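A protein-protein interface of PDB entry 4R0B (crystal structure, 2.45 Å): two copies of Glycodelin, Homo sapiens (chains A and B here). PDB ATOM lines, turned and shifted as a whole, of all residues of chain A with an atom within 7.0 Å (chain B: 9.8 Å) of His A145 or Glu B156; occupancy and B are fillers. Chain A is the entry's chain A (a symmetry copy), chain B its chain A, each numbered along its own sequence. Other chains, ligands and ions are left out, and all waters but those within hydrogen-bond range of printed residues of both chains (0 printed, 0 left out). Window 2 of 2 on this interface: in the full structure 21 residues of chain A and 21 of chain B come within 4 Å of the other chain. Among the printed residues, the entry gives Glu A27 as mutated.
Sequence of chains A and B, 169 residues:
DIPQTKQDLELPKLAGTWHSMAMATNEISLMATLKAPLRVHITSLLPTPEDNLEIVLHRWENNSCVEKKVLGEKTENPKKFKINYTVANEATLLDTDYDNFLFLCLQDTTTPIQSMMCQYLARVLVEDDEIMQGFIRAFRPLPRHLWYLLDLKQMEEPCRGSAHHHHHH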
ATOM      1  N   THR A  25      26.436  -2.969 -27.416  1.00  0.00           N
ATOM      2  CA  THR A  25      25.479  -1.979 -26.972  1.00  0.00           C
ATOM      3  C   THR A  25      24.777  -2.408 -25.687  1.00  0.00           C
ATOM      4  O   THR A  25      24.683  -3.594 -25.382  1.00  0.00           O
ATOM      5  CB  THR A  25      24.434  -1.690 -28.065  1.00  0.00           C
ATOM      6  OG1 THR A  25      23.667  -0.531 -27.703  1.00  0.00           O
ATOM      7  CG2 THR A  25      23.505  -2.886 -28.265  1.00  0.00           C
ATOM      8  N   ASN A  26      24.299  -1.415 -24.939  1.00  0.00           N
ATOM      9  CA  ASN A  26      23.444  -1.645 -23.777  1.00  0.00           C
ATOM     10  C   ASN A  26      21.964  -1.437 -24.108  1.00  0.00           C
ATOM     11  O   ASN A  26      21.122  -1.492 -23.225  1.00  0.00           O
ATOM     12  CB  ASN A  26      23.851  -0.743 -22.610  1.00  0.00           C
ATOM     13  CG  ASN A  26      23.850   0.723 -22.977  1.00  0.00           C
ATOM     14  OD1 ASN A  26      23.568   1.085 -24.121  1.00  0.00           O
ATOM     15  ND2 ASN A  26      24.185   1.575 -22.010  1.00  0.00           N
ATOM     16  N   GLU A  27      21.662  -1.184 -25.379  1.00  0.00           N
ATOM     17  CA  GLU A  27      20.291  -1.173 -25.881  1.00  0.00           C
ATOM     18  C   GLU A  27      20.275  -1.879 -27.221  1.00  0.00           C
ATOM     19  O   GLU A  27      20.717  -1.329 -28.227  1.00  0.00           O
ATOM     20  CB  GLU A  27      19.771   0.251 -26.039  1.00  0.00           C
ATOM     21  CG  GLU A  27      18.893   0.721 -24.896  1.00  0.00           C
ATOM     22  CD  GLU A  27      18.035   1.916 -25.273  1.00  0.00           C
ATOM     23  OE1 GLU A  27      18.348   2.589 -26.277  1.00  0.00           O
ATOM     24  OE2 GLU A  27      17.043   2.184 -24.563  1.00  0.00           O
ATOM     25  N   ILE A 113      20.096   7.058 -17.950  1.00  0.00           N
ATOM     26  CA  ILE A 113      20.899   5.893 -18.338  1.00  0.00           C
ATOM     27  C   ILE A 113      21.446   6.148 -19.739  1.00  0.00           C
ATOM     28  O   ILE A 113      20.689   6.198 -20.711  1.00  0.00           O
ATOM     29  CB  ILE A 113      20.084   4.582 -18.369  1.00  0.00           C
ATOM     30  CG1 ILE A 113      19.408   4.321 -17.017  1.00  0.00           C
ATOM     31  CG2 ILE A 113      20.981   3.407 -18.760  1.00  0.00           C
ATOM     32  CD1 ILE A 113      18.240   3.360 -17.101  1.00  0.00           C
ATOM     33  N   GLN A 114      22.760   6.304 -19.839  1.00  0.00           N
ATOM     34  CA  GLN A 114      23.399   6.656 -21.101  1.00  0.00           C
ATOM     35  C   GLN A 114      23.348   5.492 -22.100  1.00  0.00           C
ATOM     36  O   GLN A 114      23.969   4.452 -21.885  1.00  0.00           O
ATOM     37  CB  GLN A 114      24.841   7.091 -20.833  1.00  0.00           C
ATOM     38  CG  GLN A 114      25.664   7.415 -22.070  1.00  0.00           C
ATOM     39  CD  GLN A 114      26.931   8.187 -21.737  1.00  0.00           C
ATOM     40  OE1 GLN A 114      26.888   9.188 -21.019  1.00  0.00           O
ATOM     41  NE2 GLN A 114      28.063   7.732 -22.261  1.00  0.00           N
ATOM     42  N   MET A 116      24.238   3.746 -25.729  1.00  0.00           N
ATOM     43  CA  MET A 116      25.621   3.636 -26.153  1.00  0.00           C
ATOM     44  C   MET A 116      25.897   2.445 -27.055  1.00  0.00           C
ATOM     45  O   MET A 116      25.424   1.333 -26.796  1.00  0.00           O
ATOM     46  CB  MET A 116      26.465   3.533 -24.892  1.00  0.00           C
ATOM     47  CG  MET A 116      27.874   3.038 -25.084  1.00  0.00           C
ATOM     48  SD  MET A 116      28.871   3.439 -23.642  1.00  0.00           S
ATOM     49  CE  MET A 116      27.778   3.020 -22.284  1.00  0.00           C
ATOM     50  N   PHE A 139      33.687  -2.476 -21.547  1.00  0.00           N
ATOM     51  CA  PHE A 139      32.288  -2.133 -21.324  1.00  0.00           C
ATOM     52  C   PHE A 139      31.673  -2.839 -20.099  1.00  0.00           C
ATOM     53  O   PHE A 139      30.520  -2.607 -19.755  1.00  0.00           O
ATOM     54  CB  PHE A 139      31.459  -2.284 -22.626  1.00  0.00           C
ATOM     55  CG  PHE A 139      31.322  -3.703 -23.161  1.00  0.00           C
ATOM     56  CD1 PHE A 139      30.619  -4.694 -22.455  1.00  0.00           C
ATOM     57  CD2 PHE A 139      31.805  -4.028 -24.428  1.00  0.00           C
ATOM     58  CE1 PHE A 139      30.463  -5.980 -22.975  1.00  0.00           C
ATOM     59  CE2 PHE A 139      31.640  -5.319 -24.949  1.00  0.00           C
ATOM     60  CZ  PHE A 139      30.969  -6.288 -24.224  1.00  0.00           C
ATOM     61  N   ARG A 140      32.461  -3.662 -19.413  1.00  0.00           N
ATOM     62  CA  ARG A 140      31.981  -4.419 -18.257  1.00  0.00           C
ATOM     63  C   ARG A 140      31.743  -3.591 -16.988  1.00  0.00           C
ATOM     64  O   ARG A 140      30.624  -3.571 -16.473  1.00  0.00           O
ATOM     65  CB  ARG A 140      32.966  -5.558 -17.926  1.00  0.00           C
ATOM     66  CG  ARG A 140      32.397  -6.655 -17.024  1.00  0.00           C
ATOM     67  CD  ARG A 140      32.129  -7.964 -17.767  1.00  0.00           C
ATOM     68  NE  ARG A 140      33.264  -8.892 -17.697  1.00  0.00           N
ATOM     69  CZ  ARG A 140      33.275 -10.131 -18.195  1.00  0.00           C
ATOM     70  NH1 ARG A 140      32.215 -10.625 -18.829  1.00  0.00           N
ATOM     71  NH2 ARG A 140      34.362 -10.886 -18.059  1.00  0.00           N
ATOM     72  N   PRO A 141      32.783  -2.890 -16.493  1.00  0.00           N
ATOM     73  CA  PRO A 141      32.873  -2.602 -15.056  1.00  0.00           C
ATOM     74  C   PRO A 141      31.769  -1.695 -14.507  1.00  0.00           C
ATOM     75  O   PRO A 141      30.916  -2.167 -13.748  1.00  0.00           O
ATOM     76  CB  PRO A 141      34.261  -1.957 -14.909  1.00  0.00           C
ATOM     77  CG  PRO A 141      34.611  -1.431 -16.265  1.00  0.00           C
ATOM     78  CD  PRO A 141      33.656  -2.003 -17.278  1.00  0.00           C
ATOM     79  N   LEU A 142      31.787  -0.415 -14.882  1.00  0.00           N
ATOM     80  CA  LEU A 142      30.809   0.549 -14.374  1.00  0.00           C
ATOM     81  C   LEU A 142      29.492   0.475 -15.166  1.00  0.00           C
ATOM     82  O   LEU A 142      28.422   0.445 -14.550  1.00  0.00           O
ATOM     83  CB  LEU A 142      31.383   1.980 -14.348  1.00  0.00           C
ATOM     84  CG  LEU A 142      30.884   2.909 -13.228  1.00  0.00           C
ATOM     85  CD1 LEU A 142      31.331   2.423 -11.853  1.00  0.00           C
ATOM     86  CD2 LEU A 142      31.358   4.337 -13.467  1.00  0.00           C
ATOM     87  N   PRO A 143      29.556   0.440 -16.525  1.00  0.00           N
ATOM     88  CA  PRO A 143      28.316   0.135 -17.250  1.00  0.00           C
ATOM     89  C   PRO A 143      27.827  -1.281 -16.899  1.00  0.00           C
ATOM     90  O   PRO A 143      28.093  -2.242 -17.631  1.00  0.00           O
ATOM     91  CB  PRO A 143      28.718   0.272 -18.730  1.00  0.00           C
ATOM     92  CG  PRO A 143      29.953   1.103 -18.724  1.00  0.00           C
ATOM     93  CD  PRO A 143      30.662   0.748 -17.452  1.00  0.00           C
ATOM     94  N   ARG A 144      27.120  -1.380 -15.770  1.00  0.00           N
ATOM     95  CA  ARG A 144      26.774  -2.659 -15.147  1.00  0.00           C
ATOM     96  C   ARG A 144      25.313  -3.047 -15.402  1.00  0.00           C
ATOM     97  O   ARG A 144      24.535  -3.286 -14.472  1.00  0.00           O
ATOM     98  CB  ARG A 144      27.067  -2.602 -13.645  1.00  0.00           C
ATOM     99  CG  ARG A 144      27.302  -3.964 -13.006  1.00  0.00           C
ATOM    100  CD  ARG A 144      27.728  -3.826 -11.553  1.00  0.00           C
ATOM    101  NE  ARG A 144      28.919  -2.986 -11.409  1.00  0.00           N
ATOM    102  CZ  ARG A 144      29.422  -2.569 -10.247  1.00  0.00           C
ATOM    103  NH1 ARG A 144      28.855  -2.914  -9.094  1.00  0.00           N
ATOM    104  NH2 ARG A 144      30.506  -1.800 -10.240  1.00  0.00           N
ATOM    105  N   HIS A 145      24.967  -3.103 -16.685  1.00  0.00           N
ATOM    106  CA  HIS A 145      23.695  -3.643 -17.151  1.00  0.00           C
ATOM    107  C   HIS A 145      24.021  -4.877 -18.013  1.00  0.00           C
ATOM    108  O   HIS A 145      25.177  -5.295 -18.080  1.00  0.00           O
ATOM    109  CB  HIS A 145      22.868  -2.577 -17.913  1.00  0.00           C
ATOM    110  CG  HIS A 145      23.650  -1.364 -18.342  1.00  0.00           C
ATOM    111  ND1 HIS A 145      23.675  -0.193 -17.612  1.00  0.00           N
ATOM    112  CD2 HIS A 145      24.414  -1.134 -19.436  1.00  0.00           C
ATOM    113  CE1 HIS A 145      24.429   0.700 -18.233  1.00  0.00           C
ATOM    114  NE2 HIS A 145      24.888   0.154 -19.345  1.00  0.00           N
ATOM    115  N   LEU A 146      23.020  -5.480 -18.643  1.00  0.00           N
ATOM    116  CA  LEU A 146      23.285  -6.501 -19.646  1.00  0.00           C
ATOM    117  C   LEU A 146      23.851  -5.789 -20.874  1.00  0.00           C
ATOM    118  O   LEU A 146      23.397  -4.702 -21.235  1.00  0.00           O
ATOM    119  CB  LEU A 146      22.020  -7.258 -20.032  1.00  0.00           C
ATOM    120  CG  LEU A 146      21.265  -7.954 -18.899  1.00  0.00           C
ATOM    121  CD1 LEU A 146      19.923  -8.461 -19.401  1.00  0.00           C
ATOM    122  CD2 LEU A 146      22.075  -9.086 -18.279  1.00  0.00           C
ATOM    123  N   TRP A 147      24.851  -6.394 -21.502  1.00  0.00           N
ATOM    124  CA  TRP A 147      25.416  -5.859 -22.727  1.00  0.00           C
ATOM    125  C   TRP A 147      25.285  -6.858 -23.847  1.00  0.00           C
ATOM    126  O   TRP A 147      25.483  -8.056 -23.651  1.00  0.00           O
ATOM    127  CB  TRP A 147      26.883  -5.492 -22.530  1.00  0.00           C
ATOM    128  CG  TRP A 147      27.043  -4.092 -22.089  1.00  0.00           C
ATOM    129  CD1 TRP A 147      26.788  -3.592 -20.846  1.00  0.00           C
ATOM    130  CD2 TRP A 147      27.469  -2.987 -22.890  1.00  0.00           C
ATOM    131  NE1 TRP A 147      27.038  -2.242 -20.819  1.00  0.00           N
ATOM    132  CE2 TRP A 147      27.460  -1.843 -22.061  1.00  0.00           C
ATOM    133  CE3 TRP A 147      27.868  -2.849 -24.224  1.00  0.00           C
ATOM    134  CZ2 TRP A 147      27.838  -0.573 -22.525  1.00  0.00           C
ATOM    135  CZ3 TRP A 147      28.244  -1.581 -24.686  1.00  0.00           C
ATOM    136  CH2 TRP A 147      28.226  -0.463 -23.836  1.00  0.00           C
ATOM    137  N   SER B  20      24.476 -19.585 -15.641  1.00  0.00           N
ATOM    138  CA  SER B  20      24.699 -19.031 -16.964  1.00  0.00           C
ATOM    139  C   SER B  20      25.542 -17.781 -16.828  1.00  0.00           C
ATOM    140  O   SER B  20      25.227 -16.901 -16.013  1.00  0.00           O
ATOM    141  CB  SER B  20      23.364 -18.698 -17.639  1.00  0.00           C
ATOM    142  OG  SER B  20      22.689 -17.693 -16.907  1.00  0.00           O
ATOM    143  N   MET B  21      26.619 -17.718 -17.611  1.00  0.00           N
ATOM    144  CA  MET B  21      27.536 -16.566 -17.631  1.00  0.00           C
ATOM    145  C   MET B  21      27.354 -15.720 -18.886  1.00  0.00           C
ATOM    146  O   MET B  21      27.544 -14.503 -18.857  1.00  0.00           O
ATOM    147  CB  MET B  21      28.973 -17.062 -17.579  1.00  0.00           C
ATOM    148  CG  MET B  21      29.268 -17.953 -16.382  1.00  0.00           C
ATOM    149  SD  MET B  21      29.376 -17.024 -14.838  1.00  0.00           S
ATOM    150  CE  MET B  21      30.942 -16.184 -15.087  1.00  0.00           C
ATOM    151  N   LEU B  34      12.726 -10.822 -22.835  1.00  0.00           N
ATOM    152  CA  LEU B  34      12.413 -11.791 -21.794  1.00  0.00           C
ATOM    153  C   LEU B  34      11.367 -12.802 -22.263  1.00  0.00           C
ATOM    154  O   LEU B  34      11.396 -13.947 -21.847  1.00  0.00           O
ATOM    155  CB  LEU B  34      11.952 -11.073 -20.523  1.00  0.00           C
ATOM    156  CG  LEU B  34      13.081 -10.340 -19.784  1.00  0.00           C
ATOM    157  CD1 LEU B  34      12.534  -9.458 -18.667  1.00  0.00           C
ATOM    158  CD2 LEU B  34      14.119 -11.323 -19.241  1.00  0.00           C
ATOM    159  N   ARG B  39      15.296 -17.203 -24.471  1.00  0.00           N
ATOM    160  CA  ARG B  39      15.796 -16.414 -23.349  1.00  0.00           C
ATOM    161  C   ARG B  39      15.530 -17.212 -22.063  1.00  0.00           C
ATOM    162  O   ARG B  39      14.548 -16.972 -21.351  1.00  0.00           O
ATOM    163  CB  ARG B  39      15.156 -15.025 -23.306  1.00  0.00           C
ATOM    164  CG  ARG B  39      15.694 -14.152 -22.175  1.00  0.00           C
ATOM    165  CD  ARG B  39      17.123 -13.640 -22.384  1.00  0.00           C
ATOM    166  NE  ARG B  39      17.095 -12.323 -23.026  1.00  0.00           N
ATOM    167  CZ  ARG B  39      17.215 -11.150 -22.412  1.00  0.00           C
ATOM    168  NH1 ARG B  39      17.425 -11.068 -21.106  1.00  0.00           N
ATOM    169  NH2 ARG B  39      17.138 -10.040 -23.129  1.00  0.00           N
ATOM    170  N   HIS B  41      17.618 -19.662 -18.705  1.00  0.00           N
ATOM    171  CA  HIS B  41      18.823 -19.874 -17.907  1.00  0.00           C
ATOM    172  C   HIS B  41      18.813 -21.274 -17.344  1.00  0.00           C
ATOM    173  O   HIS B  41      17.965 -21.612 -16.511  1.00  0.00           O
ATOM    174  CB  HIS B  41      18.889 -18.855 -16.777  1.00  0.00           C
ATOM    175  CG  HIS B  41      18.981 -17.456 -17.272  1.00  0.00           C
ATOM    176  ND1 HIS B  41      20.185 -16.832 -17.520  1.00  0.00           N
ATOM    177  CD2 HIS B  41      18.018 -16.576 -17.630  1.00  0.00           C
ATOM    178  CE1 HIS B  41      19.960 -15.618 -17.984  1.00  0.00           C
ATOM    179  NE2 HIS B  41      18.653 -15.439 -18.066  1.00  0.00           N
ATOM    180  N   TRP B  60      11.560 -16.028 -17.518  1.00  0.00           N
ATOM    181  CA  TRP B  60      10.487 -15.092 -17.226  1.00  0.00           C
ATOM    182  C   TRP B  60       9.300 -15.504 -18.088  1.00  0.00           C
ATOM    183  O   TRP B  60       9.466 -15.852 -19.261  1.00  0.00           O
ATOM    184  CB  TRP B  60      10.942 -13.674 -17.555  1.00  0.00           C
ATOM    185  CG  TRP B  60       9.956 -12.583 -17.243  1.00  0.00           C
ATOM    186  CD1 TRP B  60       9.924 -11.800 -16.121  1.00  0.00           C
ATOM    187  CD2 TRP B  60       8.888 -12.118 -18.088  1.00  0.00           C
ATOM    188  NE1 TRP B  60       8.893 -10.891 -16.208  1.00  0.00           N
ATOM    189  CE2 TRP B  60       8.246 -11.062 -17.406  1.00  0.00           C
ATOM    190  CE3 TRP B  60       8.410 -12.498 -19.353  1.00  0.00           C
ATOM    191  CZ2 TRP B  60       7.142 -10.378 -17.947  1.00  0.00           C
ATOM    192  CZ3 TRP B  60       7.309 -11.819 -19.887  1.00  0.00           C
ATOM    193  CH2 TRP B  60       6.689 -10.775 -19.180  1.00  0.00           C
ATOM    194  N   LEU B 125      30.362 -18.623  -9.960  1.00  0.00           N
ATOM    195  CA  LEU B 125      30.311 -17.295 -10.599  1.00  0.00           C
ATOM    196  C   LEU B 125      31.691 -16.633 -10.646  1.00  0.00           C
ATOM    197  O   LEU B 125      32.010 -15.757  -9.826  1.00  0.00           O
ATOM    198  CB  LEU B 125      29.313 -16.393  -9.866  1.00  0.00           C
ATOM    199  CG  LEU B 125      27.879 -16.926  -9.811  1.00  0.00           C
ATOM    200  CD1 LEU B 125      27.042 -16.041  -8.900  1.00  0.00           C
ATOM    201  CD2 LEU B 125      27.266 -17.004 -11.209  1.00  0.00           C
ATOM    202  N   LEU B 150      25.045 -12.165 -25.488  1.00  0.00           N
ATOM    203  CA  LEU B 150      24.534 -11.428 -24.349  1.00  0.00           C
ATOM    204  C   LEU B 150      25.423 -11.743 -23.163  1.00  0.00           C
ATOM    205  O   LEU B 150      25.531 -12.892 -22.774  1.00  0.00           O
ATOM    206  CB  LEU B 150      23.093 -11.855 -24.088  1.00  0.00           C
ATOM    207  CG  LEU B 150      22.367 -11.292 -22.869  1.00  0.00           C
ATOM    208  CD1 LEU B 150      22.411  -9.769 -22.788  1.00  0.00           C
ATOM    209  CD2 LEU B 150      20.937 -11.807 -22.914  1.00  0.00           C
ATOM    210  N   ASP B 151      26.093 -10.730 -22.623  1.00  0.00           N
ATOM    211  CA  ASP B 151      26.995 -10.905 -21.482  1.00  0.00           C
ATOM    212  C   ASP B 151      26.250 -10.521 -20.199  1.00  0.00           C
ATOM    213  O   ASP B 151      25.924  -9.352 -19.981  1.00  0.00           O
ATOM    214  CB  ASP B 151      28.269 -10.070 -21.662  1.00  0.00           C
ATOM    215  CG  ASP B 151      29.273 -10.247 -20.503  1.00  0.00           C
ATOM    216  OD1 ASP B 151      29.390 -11.370 -19.946  1.00  0.00           O
ATOM    217  OD2 ASP B 151      29.960  -9.258 -20.145  1.00  0.00           O
ATOM    218  N   LEU B 152      25.985 -11.523 -19.360  1.00  0.00           N
ATOM    219  CA  LEU B 152      25.045 -11.395 -18.238  1.00  0.00           C
ATOM    220  C   LEU B 152      25.694 -10.745 -17.034  1.00  0.00           C
ATOM    221  O   LEU B 152      26.916 -10.651 -16.958  1.00  0.00           O
ATOM    222  CB  LEU B 152      24.494 -12.769 -17.841  1.00  0.00           C
ATOM    223  CG  LEU B 152      23.785 -13.559 -18.950  1.00  0.00           C
ATOM    224  CD1 LEU B 152      23.573 -15.008 -18.537  1.00  0.00           C
ATOM    225  CD2 LEU B 152      22.460 -12.910 -19.320  1.00  0.00           C
ATOM    226  N   LYS B 153      24.865 -10.300 -16.094  1.00  0.00           N
ATOM    227  CA  LYS B 153      25.358  -9.714 -14.849  1.00  0.00           C
ATOM    228  C   LYS B 153      24.727 -10.390 -13.630  1.00  0.00           C
ATOM    229  O   LYS B 153      23.790 -11.179 -13.761  1.00  0.00           O
ATOM    230  CB  LYS B 153      25.130  -8.197 -14.842  1.00  0.00           C
ATOM    231  CG  LYS B 153      25.862  -7.457 -15.962  1.00  0.00           C
ATOM    232  CD  LYS B 153      27.384  -7.479 -15.806  1.00  0.00           C
ATOM    233  CE  LYS B 153      28.115  -7.533 -17.148  1.00  0.00           C
ATOM    234  NZ  LYS B 153      27.931  -6.312 -17.985  1.00  0.00           N
ATOM    235  N   GLN B 154      25.261 -10.079 -12.448  1.00  0.00           N
ATOM    236  CA  GLN B 154      24.930 -10.804 -11.215  1.00  0.00           C
ATOM    237  C   GLN B 154      23.644 -10.277 -10.581  1.00  0.00           C
ATOM    238  O   GLN B 154      23.593  -9.137 -10.113  1.00  0.00           O
ATOM    239  CB  GLN B 154      26.079 -10.717 -10.197  1.00  0.00           C
ATOM    240  CG  GLN B 154      27.349 -11.460 -10.602  1.00  0.00           C
ATOM    241  CD  GLN B 154      28.145 -10.737 -11.676  1.00  0.00           C
ATOM    242  OE1 GLN B 154      28.386  -9.532 -11.585  1.00  0.00           O
ATOM    243  NE2 GLN B 154      28.555 -11.471 -12.705  1.00  0.00           N
ATOM    244  N   MET B 155      22.615 -11.125 -10.567  1.00  0.00           N
ATOM    245  CA  MET B 155      21.290 -10.775 -10.044  1.00  0.00           C
ATOM    246  C   MET B 155      20.746  -9.460 -10.618  1.00  0.00           C
ATOM    247  O   MET B 155      20.064  -8.701  -9.924  1.00  0.00           O
ATOM    248  CB  MET B 155      21.291 -10.756  -8.502  1.00  0.00           C
ATOM    249  CG  MET B 155      21.094 -12.121  -7.848  1.00  0.00           C
ATOM    250  SD  MET B 155      19.644 -13.047  -8.411  1.00  0.00           S
ATOM    251  CE  MET B 155      18.392 -11.767  -8.511  1.00  0.00           C
ATOM    252  N   GLU B 156      21.058  -9.199 -11.886  1.00  0.00           N
ATOM    253  CA  GLU B 156      20.405  -8.138 -12.643  1.00  0.00           C
ATOM    254  C   GLU B 156      19.272  -8.765 -13.446  1.00  0.00           C
ATOM    255  O   GLU B 156      18.167  -8.223 -13.494  1.00  0.00           O
ATOM    256  CB  GLU B 156      21.385  -7.446 -13.585  1.00  0.00           C
ATOM    257  CG  GLU B 156      20.857  -6.123 -14.129  1.00  0.00           C
ATOM    258  CD  GLU B 156      21.398  -5.777 -15.503  1.00  0.00           C
ATOM    259  OE1 GLU B 156      20.830  -4.867 -16.143  1.00  0.00           O
ATOM    260  OE2 GLU B 156      22.383  -6.407 -15.946  1.00  0.00           O
ATOM    261  N   GLU B 157      19.562  -9.899 -14.085  1.00  0.00           N
ATOM    262  CA  GLU B 157      18.536 -10.704 -14.743  1.00  0.00           C
ATOM    263  C   GLU B 157      17.590 -11.258 -13.666  1.00  0.00           C
ATOM    264  O   GLU B 157      18.057 -11.881 -12.706  1.00  0.00           O
ATOM    265  CB  GLU B 157      19.178 -11.845 -15.536  1.00  0.00           C
ATOM    266  CG  GLU B 157      18.206 -12.640 -16.403  1.00  0.00           C
ATOM    267  CD  GLU B 157      17.999 -12.056 -17.793  1.00  0.00           C
ATOM    268  OE1 GLU B 157      18.172 -10.835 -17.980  1.00  0.00           O
ATOM    269  OE2 GLU B 157      17.655 -12.831 -18.706  1.00  0.00           O
ATOM    270  N   PRO B 158      16.265 -11.035 -13.819  1.00  0.00           N
ATOM    271  CA  PRO B 158      15.313 -11.344 -12.737  1.00  0.00           C
ATOM    272  C   PRO B 158      15.247 -12.814 -12.312  1.00  0.00           C
ATOM    273  O   PRO B 158      14.945 -13.101 -11.150  1.00  0.00           O
ATOM    274  CB  PRO B 158      13.956 -10.910 -13.320  1.00  0.00           C
ATOM    275  CG  PRO B 158      14.279 -10.009 -14.461  1.00  0.00           C
ATOM    276  CD  PRO B 158      15.570 -10.522 -15.014  1.00  0.00           C
ATOM    277  N   CYS B 159      15.533 -13.724 -13.245  1.00  0.00           N
ATOM    278  CA  CYS B 159      15.378 -15.156 -13.013  1.00  0.00           C
ATOM    279  C   CYS B 159      16.583 -15.945 -13.536  1.00  0.00           C
ATOM    280  O   CYS B 159      17.083 -16.861 -12.876  1.00  0.00           O
ATOM    281  CB  CYS B 159      14.098 -15.626 -13.701  1.00  0.00           C
ATOM    282  SG  CYS B 159      13.582 -17.307 -13.289  1.00  0.00           S
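Printed residues of chain B that touch a printed residue of chain A: Arg B39, Leu B150, Asp B151, Leu B152, Lys B153, Glu B156 and Glu B157.
Hydrophobic or aromatic side chains of chain B that line the printed part of chain A: Leu B150 and Leu B152.
Of the 15 printed residues of chain A, 4 touch a printed residue of chain B.
Hydrophobic or aromatic side chains of chain A within 4 Å of the printed part of chain B: His A145 and Leu A146.
OD2 of Asp B151 lies within salt-bridge range of NH1 of Arg A140, at 2.9 Å.
The backbone carbonyl oxygen (O) of Trp A147 sits at hydrogen-bond distance from the backbone NH (N) of Asp B151, 2.9 Å away.
NZ of Lys B153 lies within hydrogen-bond range of O of His A145.
OE2 of Glu B156 is in hydrogen-bond range of N of Leu A146 (2.9 Å).
Met A116 touches none of the printed residues of chain B.
Of the printed residues of chain B, Arg A140 touches Asp B151 (2.9 Å).
Of the printed residues of chain B, Leu A146 touches Arg B39 (3.99 Å), Leu B150 (3.7 Å), Asp B151 (3.9 Å), Leu B152 (3.8 Å), Lys B153 (3.7 Å), Glu B156 (2.9 Å) and Glu B157 (3.3 Å).
Met B21 touches none of the printed residues of chain A.
Of the printed residues of chain A, Leu B150 touches Leu A146 and Trp A147.
Of the printed residues of chain A, Asp B151 touches Arg A140 (2.9 Å), Leu A146 (3.9 Å) and Trp A147 (2.9 Å).
Printed residues of chain A within 4 Å of Leu B152: Leu A146.
Of chain A, only His A145 (3.0 Å) and Leu A146 (2.9 Å) come within 4 Å of Glu B156.
The nearest residue of chain A that does not touch Glu B156 is Arg A144 (4.1 Å).
Among the printed residues, merely in contact across the chains: His A145 with Glu B156 (3.0 Å), Leu A146 with Glu B157 (3.3 Å), Trp A147 with Leu B150 (3.6 Å), Leu A146 with Lys B153 (3.7 Å), Leu A146 with Leu B150 (3.7 Å), Leu A146 with Leu B152 (3.8 Å), Leu A146 with Asp B151 (3.9 Å) and Leu A146 with Arg B39 (3.99 Å).
O of Met B21 is in hydrogen-bond range of N of Leu B152, at 3.4 Å.
OE2 of Glu B157 lies within salt-bridge range of NH1 of Arg B39, at 3.0 Å.
NE2 of His B41 lies within hydrogen-bond range of OE2 of Glu B157 (2.9 Å).
The side-chain amide nitrogen (ND2) of Asn A26 sits at hydrogen-bond distance from a ring nitrogen (NE2) of His A145.
The backbone carbonyl oxygen (O) of Pro A143 is in hydrogen-bond range of the indole nitrogen (NE1) of Trp A147 (3.4 Å).
No position is printed for both chains.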
